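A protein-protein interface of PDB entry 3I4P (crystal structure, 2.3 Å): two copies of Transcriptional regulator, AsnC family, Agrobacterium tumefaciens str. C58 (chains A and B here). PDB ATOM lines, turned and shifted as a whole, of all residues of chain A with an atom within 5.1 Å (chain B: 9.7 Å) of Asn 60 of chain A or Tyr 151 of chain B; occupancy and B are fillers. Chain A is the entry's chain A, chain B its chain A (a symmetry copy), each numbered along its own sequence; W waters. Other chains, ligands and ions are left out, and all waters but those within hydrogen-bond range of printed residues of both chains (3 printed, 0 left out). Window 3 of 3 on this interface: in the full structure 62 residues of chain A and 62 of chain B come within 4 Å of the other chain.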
ATOM      1  N   PRO A  56     -13.489   5.235   0.185  1.00  0.00           N
ATOM      2  CA  PRO A  56     -12.523   4.636   1.118  1.00  0.00           C
ATOM      3  C   PRO A  56     -12.059   3.228   0.710  1.00  0.00           C
ATOM      4  O   PRO A  56     -10.897   2.870   0.941  1.00  0.00           O
ATOM      5  CB  PRO A  56     -13.293   4.594   2.438  1.00  0.00           C
ATOM      6  CG  PRO A  56     -14.753   4.743   2.065  1.00  0.00           C
ATOM      7  CD  PRO A  56     -14.780   5.568   0.833  1.00  0.00           C
ATOM      8  N   VAL A  57     -12.956   2.449   0.101  1.00  0.00           N
ATOM      9  CA  VAL A  57     -12.580   1.130  -0.434  1.00  0.00           C
ATOM     10  C   VAL A  57     -11.515   1.270  -1.538  1.00  0.00           C
ATOM     11  O   VAL A  57     -10.607   0.471  -1.607  1.00  0.00           O
ATOM     12  CB  VAL A  57     -13.818   0.338  -0.930  1.00  0.00           C
ATOM     13  CG1 VAL A  57     -13.408  -0.905  -1.688  1.00  0.00           C
ATOM     14  CG2 VAL A  57     -14.743   0.012   0.263  1.00  0.00           C
ATOM     15  N   LYS A  58     -11.601   2.316  -2.362  1.00  0.00           N
ATOM     16  CA  LYS A  58     -10.674   2.500  -3.466  1.00  0.00           C
ATOM     17  C   LYS A  58      -9.372   3.175  -3.077  1.00  0.00           C
ATOM     18  O   LYS A  58      -8.405   3.044  -3.775  1.00  0.00           O
ATOM     19  CB  LYS A  58     -11.341   3.257  -4.629  1.00  0.00           C
ATOM     20  CG  LYS A  58     -12.320   2.385  -5.404  1.00  0.00           C
ATOM     21  CD  LYS A  58     -13.216   3.201  -6.344  1.00  0.00           C
ATOM     22  CE  LYS A  58     -14.456   2.418  -6.775  1.00  0.00           C
ATOM     23  NZ  LYS A  58     -14.102   1.083  -7.328  1.00  0.00           N
ATOM     24  N   VAL A  59      -9.302   3.881  -1.965  1.00  0.00           N
ATOM     25  CA  VAL A  59      -7.993   4.421  -1.524  1.00  0.00           C
ATOM     26  C   VAL A  59      -7.414   3.598  -0.365  1.00  0.00           C
ATOM     27  O   VAL A  59      -6.479   4.018   0.306  1.00  0.00           O
ATOM     28  CB  VAL A  59      -8.055   5.946  -1.207  1.00  0.00           C
ATOM     29  CG1 VAL A  59      -8.389   6.711  -2.464  1.00  0.00           C
ATOM     30  CG2 VAL A  59      -9.026   6.251  -0.022  1.00  0.00           C
ATOM     31  N   ASN A  60      -7.976   2.419  -0.145  1.00  0.00           N
ATOM     32  CA  ASN A  60      -7.459   1.454   0.852  1.00  0.00           C
ATOM     33  C   ASN A  60      -7.520   1.937   2.312  1.00  0.00           C
ATOM     34  O   ASN A  60      -6.605   1.703   3.105  1.00  0.00           O
ATOM     35  CB  ASN A  60      -6.033   0.994   0.471  1.00  0.00           C
ATOM     36  CG  ASN A  60      -5.631  -0.305   1.156  1.00  0.00           C
ATOM     37  OD1 ASN A  60      -6.479  -1.148   1.482  1.00  0.00           O
ATOM     38  ND2 ASN A  60      -4.331  -0.469   1.390  1.00  0.00           N
ATOM     39  N   THR A  61      -8.612   2.595   2.656  1.00  0.00           N
ATOM     40  CA  THR A  61      -8.880   3.010   4.040  1.00  0.00           C
ATOM     41  C   THR A  61     -10.277   2.548   4.490  1.00  0.00           C
ATOM     42  O   THR A  61     -11.055   3.340   5.057  1.00  0.00           O
ATOM     43  CB  THR A  61      -8.751   4.525   4.177  1.00  0.00           C
ATOM     44  OG1 THR A  61      -9.815   5.139   3.468  1.00  0.00           O
ATOM     45  CG2 THR A  61      -7.427   5.010   3.594  1.00  0.00           C
ATOM     46  N   LYS A  62     -10.578   1.261   4.271  1.00  0.00           N
ATOM     47  CA  LYS A  62     -11.957   0.729   4.398  1.00  0.00           C
ATOM     48  C   LYS A  62     -12.413   0.416   5.815  1.00  0.00           C
ATOM     49  O   LYS A  62     -13.603   0.184   6.024  1.00  0.00           O
ATOM     50  CB  LYS A  62     -12.163  -0.530   3.529  1.00  0.00           C
ATOM     51  CG  LYS A  62     -11.525  -1.802   4.077  1.00  0.00           C
ATOM     52  CD  LYS A  62     -11.410  -2.953   3.027  1.00  0.00           C
ATOM     53  CE  LYS A  62     -10.607  -4.181   3.587  1.00  0.00           C
ATOM     54  NZ  LYS A  62      -9.085  -3.986   3.803  1.00  0.00           N
ATOM     55  N   GLU A  91      -4.900   9.821   9.677  1.00  0.00           N
ATOM     56  CA  GLU A  91      -5.872   8.803   9.941  1.00  0.00           C
ATOM     57  C   GLU A  91      -6.945   9.248  10.920  1.00  0.00           C
ATOM     58  O   GLU A  91      -7.959   8.598  10.972  1.00  0.00           O
ATOM     59  CB  GLU A  91      -5.254   7.509  10.505  1.00  0.00           C
ATOM     60  CG  GLU A  91      -4.233   6.878   9.611  1.00  0.00           C
ATOM     61  CD  GLU A  91      -2.805   7.407   9.843  1.00  0.00           C
ATOM     62  OE1 GLU A  91      -2.605   8.411  10.575  1.00  0.00           O
ATOM     63  OE2 GLU A  91      -1.876   6.802   9.258  1.00  0.00           O
ATOM     64  N   VAL A 109      -9.520   5.942  10.292  1.00  0.00           N
ATOM     65  CA  VAL A 109      -9.657   5.073   9.104  1.00  0.00           C
ATOM     66  C   VAL A 109      -8.266   4.492   8.688  1.00  0.00           C
ATOM     67  O   VAL A 109      -7.230   5.185   8.692  1.00  0.00           O
ATOM     68  CB  VAL A 109     -10.398   5.801   7.928  1.00  0.00           C
ATOM     69  CG1 VAL A 109     -11.858   6.226   8.365  1.00  0.00           C
ATOM     70  CG2 VAL A 109      -9.622   7.000   7.475  1.00  0.00           C
ATOM     71  N   VAL A 110      -8.287   3.200   8.345  1.00  0.00           N
ATOM     72  CA  VAL A 110      -7.110   2.398   8.029  1.00  0.00           C
ATOM     73  C   VAL A 110      -7.599   1.245   7.122  1.00  0.00           C
ATOM     74  O   VAL A 110      -8.814   0.994   7.040  1.00  0.00           O
ATOM     75  CB  VAL A 110      -6.403   1.842   9.326  1.00  0.00           C
ATOM     76  CG1 VAL A 110      -5.675   2.959  10.090  1.00  0.00           C
ATOM     77  CG2 VAL A 110      -7.381   1.101  10.236  1.00  0.00           C
ATOM     78  N   PRO A 111      -6.663   0.534   6.441  1.00  0.00           N
ATOM     79  CA  PRO A 111      -7.071  -0.636   5.618  1.00  0.00           C
ATOM     80  C   PRO A 111      -7.445  -1.890   6.419  1.00  0.00           C
ATOM     81  O   PRO A 111      -8.284  -2.682   5.969  1.00  0.00           O
ATOM     82  CB  PRO A 111      -5.835  -0.919   4.758  1.00  0.00           C
ATOM     83  CG  PRO A 111      -4.687  -0.306   5.538  1.00  0.00           C
ATOM     84  CD  PRO A 111      -5.264   0.919   6.188  1.00  0.00           C
ATOM     85  N   ALA A 115      -2.753  -2.283  10.255  1.00  0.00           N
ATOM     86  CA  ALA A 115      -2.563  -0.839  10.024  1.00  0.00           C
ATOM     87  C   ALA A 115      -3.052  -0.037  11.246  1.00  0.00           C
ATOM     88  O   ALA A 115      -2.488   0.975  11.586  1.00  0.00           O
ATOM     89  CB  ALA A 115      -3.305  -0.362   8.750  1.00  0.00           C
ATOM     90  N   PHE A 119      -0.826   2.355  13.742  1.00  0.00           N
ATOM     91  CA  PHE A 119      -1.244   3.754  13.931  1.00  0.00           C
ATOM     92  C   PHE A 119      -1.243   4.067  15.435  1.00  0.00           C
ATOM     93  O   PHE A 119      -0.663   5.057  15.887  1.00  0.00           O
ATOM     94  CB  PHE A 119      -2.644   4.038  13.335  1.00  0.00           C
ATOM     95  CG  PHE A 119      -3.360   5.194  14.026  1.00  0.00           C
ATOM     96  CD1 PHE A 119      -3.025   6.510  13.734  1.00  0.00           C
ATOM     97  CD2 PHE A 119      -4.310   4.953  15.026  1.00  0.00           C
ATOM     98  CE1 PHE A 119      -3.628   7.578  14.416  1.00  0.00           C
ATOM     99  CE2 PHE A 119      -4.931   6.012  15.709  1.00  0.00           C
ATOM    100  CZ  PHE A 119      -4.599   7.327  15.401  1.00  0.00           C
ATOM    101  N   ARG A 122       2.104   4.611  16.935  1.00  0.00           N
ATOM    102  CA  ARG A 122       2.628   5.945  16.655  1.00  0.00           C
ATOM    103  C   ARG A 122       1.947   6.990  17.528  1.00  0.00           C
ATOM    104  O   ARG A 122       2.613   7.856  18.072  1.00  0.00           O
ATOM    105  CB  ARG A 122       2.510   6.334  15.175  1.00  0.00           C
ATOM    106  CG  ARG A 122       3.397   5.533  14.236  1.00  0.00           C
ATOM    107  CD  ARG A 122       3.377   6.027  12.771  1.00  0.00           C
ATOM    108  NE  ARG A 122       2.023   6.285  12.246  1.00  0.00           N
ATOM    109  CZ  ARG A 122       1.267   5.403  11.572  1.00  0.00           C
ATOM    110  NH1 ARG A 122       1.690   4.151  11.305  1.00  0.00           N
ATOM    111  NH2 ARG A 122       0.047   5.769  11.173  1.00  0.00           N
ATOM    112  N   MET B   1      -3.987   4.798  -7.964  1.00  0.00           N
ATOM    113  CA  MET B   1      -3.206   4.099  -9.038  1.00  0.00           C
ATOM    114  C   MET B   1      -1.692   4.301  -8.987  1.00  0.00           C
ATOM    115  O   MET B   1      -0.965   3.354  -8.741  1.00  0.00           O
ATOM    116  CB  MET B   1      -3.713   4.503 -10.417  1.00  0.00           C
ATOM    117  CG  MET B   1      -4.447   3.409 -11.143  1.00  0.00           C
ATOM    118  SD  MET B   1      -3.280   1.919 -11.293  1.00  0.00           S
ATOM    119  CE  MET B   1      -3.540   1.002  -9.514  1.00  0.00           C
ATOM    120  N   ARG B   6      -2.047  10.200  -6.658  1.00  0.00           N
ATOM    121  CA  ARG B   6      -2.082  10.581  -5.259  1.00  0.00           C
ATOM    122  C   ARG B   6      -1.901  12.099  -5.030  1.00  0.00           C
ATOM    123  O   ARG B   6      -2.652  12.692  -4.214  1.00  0.00           O
ATOM    124  CB  ARG B   6      -1.053   9.795  -4.465  1.00  0.00           C
ATOM    125  CG  ARG B   6      -1.136  10.048  -2.959  1.00  0.00           C
ATOM    126  CD  ARG B   6       0.099   9.554  -2.263  1.00  0.00           C
ATOM    127  NE  ARG B   6      -0.070   8.209  -1.773  1.00  0.00           N
ATOM    128  CZ  ARG B   6       0.906   7.320  -1.641  1.00  0.00           C
ATOM    129  NH1 ARG B   6       2.154   7.602  -2.013  1.00  0.00           N
ATOM    130  NH2 ARG B   6       0.607   6.115  -1.166  1.00  0.00           N
ATOM    131  N   LEU B   9      -5.202  13.753  -6.039  1.00  0.00           N
ATOM    132  CA  LEU B   9      -6.209  13.491  -5.000  1.00  0.00           C
ATOM    133  C   LEU B   9      -5.970  14.253  -3.704  1.00  0.00           C
ATOM    134  O   LEU B   9      -6.926  14.679  -3.029  1.00  0.00           O
ATOM    135  CB  LEU B   9      -6.313  11.991  -4.699  1.00  0.00           C
ATOM    136  CG  LEU B   9      -6.836  11.118  -5.844  1.00  0.00           C
ATOM    137  CD1 LEU B   9      -6.750   9.626  -5.478  1.00  0.00           C
ATOM    138  CD2 LEU B   9      -8.239  11.542  -6.290  1.00  0.00           C
ATOM    139  N   ARG B  10      -4.711  14.438  -3.347  1.00  0.00           N
ATOM    140  CA  ARG B  10      -4.391  15.152  -2.109  1.00  0.00           C
ATOM    141  C   ARG B  10      -4.879  16.608  -2.150  1.00  0.00           C
ATOM    142  O   ARG B  10      -5.339  17.160  -1.129  1.00  0.00           O
ATOM    143  CB  ARG B  10      -2.901  15.076  -1.874  1.00  0.00           C
ATOM    144  CG  ARG B  10      -2.361  15.799  -0.657  1.00  0.00           C
ATOM    145  CD  ARG B  10      -0.891  15.234  -0.395  1.00  0.00           C
ATOM    146  NE  ARG B  10      -0.955  13.906   0.252  1.00  0.00           N
ATOM    147  CZ  ARG B  10      -0.180  12.851  -0.005  1.00  0.00           C
ATOM    148  NH1 ARG B  10       0.788  12.903  -0.940  1.00  0.00           N
ATOM    149  NH2 ARG B  10      -0.360  11.721   0.695  1.00  0.00           N
ATOM    150  N   VAL B  46     -13.082   6.363  -7.867  1.00  0.00           N
ATOM    151  CA  VAL B  46     -12.115   6.745  -6.817  1.00  0.00           C
ATOM    152  C   VAL B  46     -12.527   8.094  -6.225  1.00  0.00           C
ATOM    153  O   VAL B  46     -12.689   8.217  -5.022  1.00  0.00           O
ATOM    154  CB  VAL B  46     -10.671   6.802  -7.355  1.00  0.00           C
ATOM    155  CG1 VAL B  46      -9.725   7.278  -6.274  1.00  0.00           C
ATOM    156  CG2 VAL B  46     -10.235   5.434  -7.904  1.00  0.00           C
ATOM    157  N   LEU B 147      -9.387  11.639   3.438  1.00  0.00           N
ATOM    158  CA  LEU B 147      -8.861  10.347   3.820  1.00  0.00           C
ATOM    159  C   LEU B 147      -7.316  10.372   3.839  1.00  0.00           C
ATOM    160  O   LEU B 147      -6.691  11.123   3.108  1.00  0.00           O
ATOM    161  CB  LEU B 147      -9.389   9.260   2.865  1.00  0.00           C
ATOM    162  CG  LEU B 147     -10.937   9.112   2.824  1.00  0.00           C
ATOM    163  CD1 LEU B 147     -11.358   8.090   1.774  1.00  0.00           C
ATOM    164  CD2 LEU B 147     -11.528   8.771   4.238  1.00  0.00           C
ATOM    165  N   PRO B 148      -6.697   9.523   4.686  1.00  0.00           N
ATOM    166  CA  PRO B 148      -5.232   9.334   4.596  1.00  0.00           C
ATOM    167  C   PRO B 148      -4.891   8.643   3.287  1.00  0.00           C
ATOM    168  O   PRO B 148      -5.584   7.684   2.891  1.00  0.00           O
ATOM    169  CB  PRO B 148      -4.914   8.438   5.814  1.00  0.00           C
ATOM    170  CG  PRO B 148      -6.216   7.716   6.143  1.00  0.00           C
ATOM    171  CD  PRO B 148      -7.323   8.686   5.748  1.00  0.00           C
ATOM    172  N   LEU B 149      -3.872   9.141   2.583  1.00  0.00           N
ATOM    173  CA  LEU B 149      -3.574   8.655   1.251  1.00  0.00           C
ATOM    174  C   LEU B 149      -2.279   7.823   1.241  1.00  0.00           C
ATOM    175  O   LEU B 149      -1.880   7.300   0.188  1.00  0.00           O
ATOM    176  CB  LEU B 149      -3.552   9.817   0.239  1.00  0.00           C
ATOM    177  CG  LEU B 149      -4.868  10.607   0.105  1.00  0.00           C
ATOM    178  CD1 LEU B 149      -4.703  11.796  -0.827  1.00  0.00           C
ATOM    179  CD2 LEU B 149      -5.982   9.714  -0.379  1.00  0.00           C
ATOM    180  N   ASP B 150      -1.676   7.673   2.424  1.00  0.00           N
ATOM    181  CA  ASP B 150      -0.474   6.875   2.605  1.00  0.00           C
ATOM    182  C   ASP B 150      -0.689   5.369   2.333  1.00  0.00           C
ATOM    183  O   ASP B 150       0.262   4.666   2.121  1.00  0.00           O
ATOM    184  CB  ASP B 150       0.108   7.105   4.016  1.00  0.00           C
ATOM    185  N   TYR B 151      -1.922   4.880   2.291  1.00  0.00           N
ATOM    186  CA  TYR B 151      -2.180   3.440   2.149  1.00  0.00           C
ATOM    187  C   TYR B 151      -2.573   3.009   0.735  1.00  0.00           C
ATOM    188  O   TYR B 151      -2.748   1.808   0.469  1.00  0.00           O
ATOM    189  CB  TYR B 151      -3.317   3.049   3.104  1.00  0.00           C
ATOM    190  CG  TYR B 151      -3.022   3.377   4.556  1.00  0.00           C
ATOM    191  CD1 TYR B 151      -2.138   2.579   5.304  1.00  0.00           C
ATOM    192  CD2 TYR B 151      -3.583   4.476   5.173  1.00  0.00           C
ATOM    193  CE1 TYR B 151      -1.854   2.859   6.636  1.00  0.00           C
ATOM    194  CE2 TYR B 151      -3.298   4.771   6.512  1.00  0.00           C
ATOM    195  CZ  TYR B 151      -2.435   3.942   7.235  1.00  0.00           C
ATOM    196  OH  TYR B 151      -2.154   4.208   8.552  1.00  0.00           O
ATOM    197  N   MET B 152      -2.773   3.999  -0.139  1.00  0.00           N
ATOM    198  CA  MET B 152      -3.220   3.783  -1.520  1.00  0.00           C
ATOM    199  C   MET B 152      -2.344   2.768  -2.242  1.00  0.00           C
ATOM    200  O   MET B 152      -1.097   2.735  -2.058  1.00  0.00           O
ATOM    201  CB  MET B 152      -3.149   5.077  -2.327  1.00  0.00           C
ATOM    202  CG  MET B 152      -4.266   5.972  -2.138  1.00  0.00           C
ATOM    203  SD  MET B 152      -4.087   7.512  -3.289  1.00  0.00           S
ATOM    204  CE  MET B 152      -4.437   6.653  -5.000  1.00  0.00           C
ATOM    205  N   LEU B 153      -2.980   1.949  -3.081  1.00  0.00           N
ATOM    206  CA  LEU B 153      -2.261   0.799  -3.689  1.00  0.00           C
ATOM    207  C   LEU B 153      -2.930   0.318  -4.974  1.00  0.00           C
ATOM    208  O   LEU B 153      -2.598   0.799  -6.054  1.00  0.00           O
ATOM    209  CB  LEU B 153      -2.114  -0.341  -2.646  1.00  0.00           C
ATOM    210  CG  LEU B 153      -0.713  -0.660  -2.069  1.00  0.00           C
ATOM    211  CD1 LEU B 153       0.427   0.252  -2.670  1.00  0.00           C
ATOM    212  CD2 LEU B 153      -0.698  -0.679  -0.525  1.00  0.00           C
HETATM  213  O   HOH W   1      -0.835   2.359   9.883  1.00  0.00           O
HETATM  214  O   HOH W   2      -5.972   1.602  -3.074  1.00  0.00           O
HETATM  215  O   HOH W   3      -4.856   5.643   1.672  1.00  0.00           O
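Water W3 lies within hydrogen-bond range of O of Pro 148 of chain B (2.5 Å), O of Val 59 of chain A (2.7 Å), N of Tyr 151 of chain B (3.1 Å) and N of Met 152 of chain B (3.2 Å).
Water W1 lies within hydrogen-bond range of the side-chain hydroxyl of Tyr 151 of chain B (2.6 Å), the backbone carbonyl oxygen of Ala 115 of chain A (2.7 Å) and the guanidinium group of Arg 122 of chain A (3.4 Å).
Water W2 lies within hydrogen-bond range of the backbone carbonyl oxygen (O) of Lys 58 of chain A (2.9 Å) and the backbone NH (N) of Leu 153 of chain B (3.0 Å).
The side-chain amide nitrogen (ND2) of Asn 60 of chain A is in hydrogen-bond range of the backbone carbonyl oxygen (O) of Tyr 151 of chain B (2.9 Å).
The side-chain carboxylate of Glu 91 of chain A is in hydrogen-bond range of the side-chain hydroxyl of Tyr 151 of chain B (2.7 Å).
Among the printed residues, pairs that only touch across the chains: Pro 56 of chain A with Leu 147 of chain B (3.7 Å), Lys 58 of chain A with Val 46 of chain B (3.5 Å), Val 59 of chain A with Leu 147 of chain B (3.5 Å), Val 59 of chain A with Met 152 of chain B (3.7 Å), Thr 61 of chain A with Leu 147 of chain B (3.7 Å), Thr 61 of chain A with Pro 148 of chain B (3.3 Å), Glu 91 of chain A with Pro 148 of chain B (3.97 Å), Val 109 of chain A with Pro 148 of chain B (3.3 Å), Pro 111 of chain A with Tyr 151 of chain B (3.6 Å) and Arg 122 of chain A with Tyr 151 of chain B (3.8 Å).
Asn 60 of chain A touches one residue of chain B.
Tyr 151 of chain B touches just these residues of chain A: Asn 60, Glu 91, Pro 111 and Arg 122.
Thr 61 of chain A touches two residues of chain B.
Pro 111 of chain A touches just one residue of chain B: Tyr 151 (3.6 Å).
Of the printed residues of chain A, Val 46 of chain B touches Lys 58 (3.5 Å).
Of the printed residues of chain A, Pro 148 of chain B touches Thr 61, Glu 91 and Val 109.
Printed residues of chain B within 4 Å of Arg 122 of chain A: Tyr 151 (3.8 Å).
Printed residues of chain B within 4 Å of Glu 91 of chain A: Pro 148 and Tyr 151.
Val 110 of chain A touches none of the printed residues of chain B.
Arg 10 of chain B touches none of the printed residues of chain A.
The nearest printed residue of chain A that does not touch Tyr 151 of chain B is Val 110 of chain A (4.04 Å).
The nearest printed residue of chain B that does not touch Arg 122 of chain A is Asp 150 of chain B (7.3 Å).
Hydrophobic or aromatic side chains of chain A that line the printed part of chain B: Val 59, Val 109 and Pro 111.
Of the 12 printed residues of chain B, 5 touch a printed residue of chain A.
Along chain B the printed residues that touch a printed residue of chain A span positions 46 to 152.
Among the printed residues, 12 pairs touch across the chains.
Among the printed residues, no Asp or Glu carboxylate lies within 4 Å of a Lys or Arg side-chain nitrogen of the other chain.
No position is printed for both chains.
NH2 of Arg 122 of chain A lies within salt-bridge range of OE2 of Glu 91 of chain A, at 2.9 Å.
The side-chain amino group (NZ) of Lys 62 of chain A is in hydrogen-bond range of the backbone carbonyl oxygen (O) of Pro 111 of chain A (2.7 Å).
O of Pro 56 of chain A lies within hydrogen-bond range of N of Thr 61 of chain A (2.9 Å).
O of Glu 91 of chain A sits at hydrogen-bond distance from N of Val 109 of chain A, 3.2 Å away.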
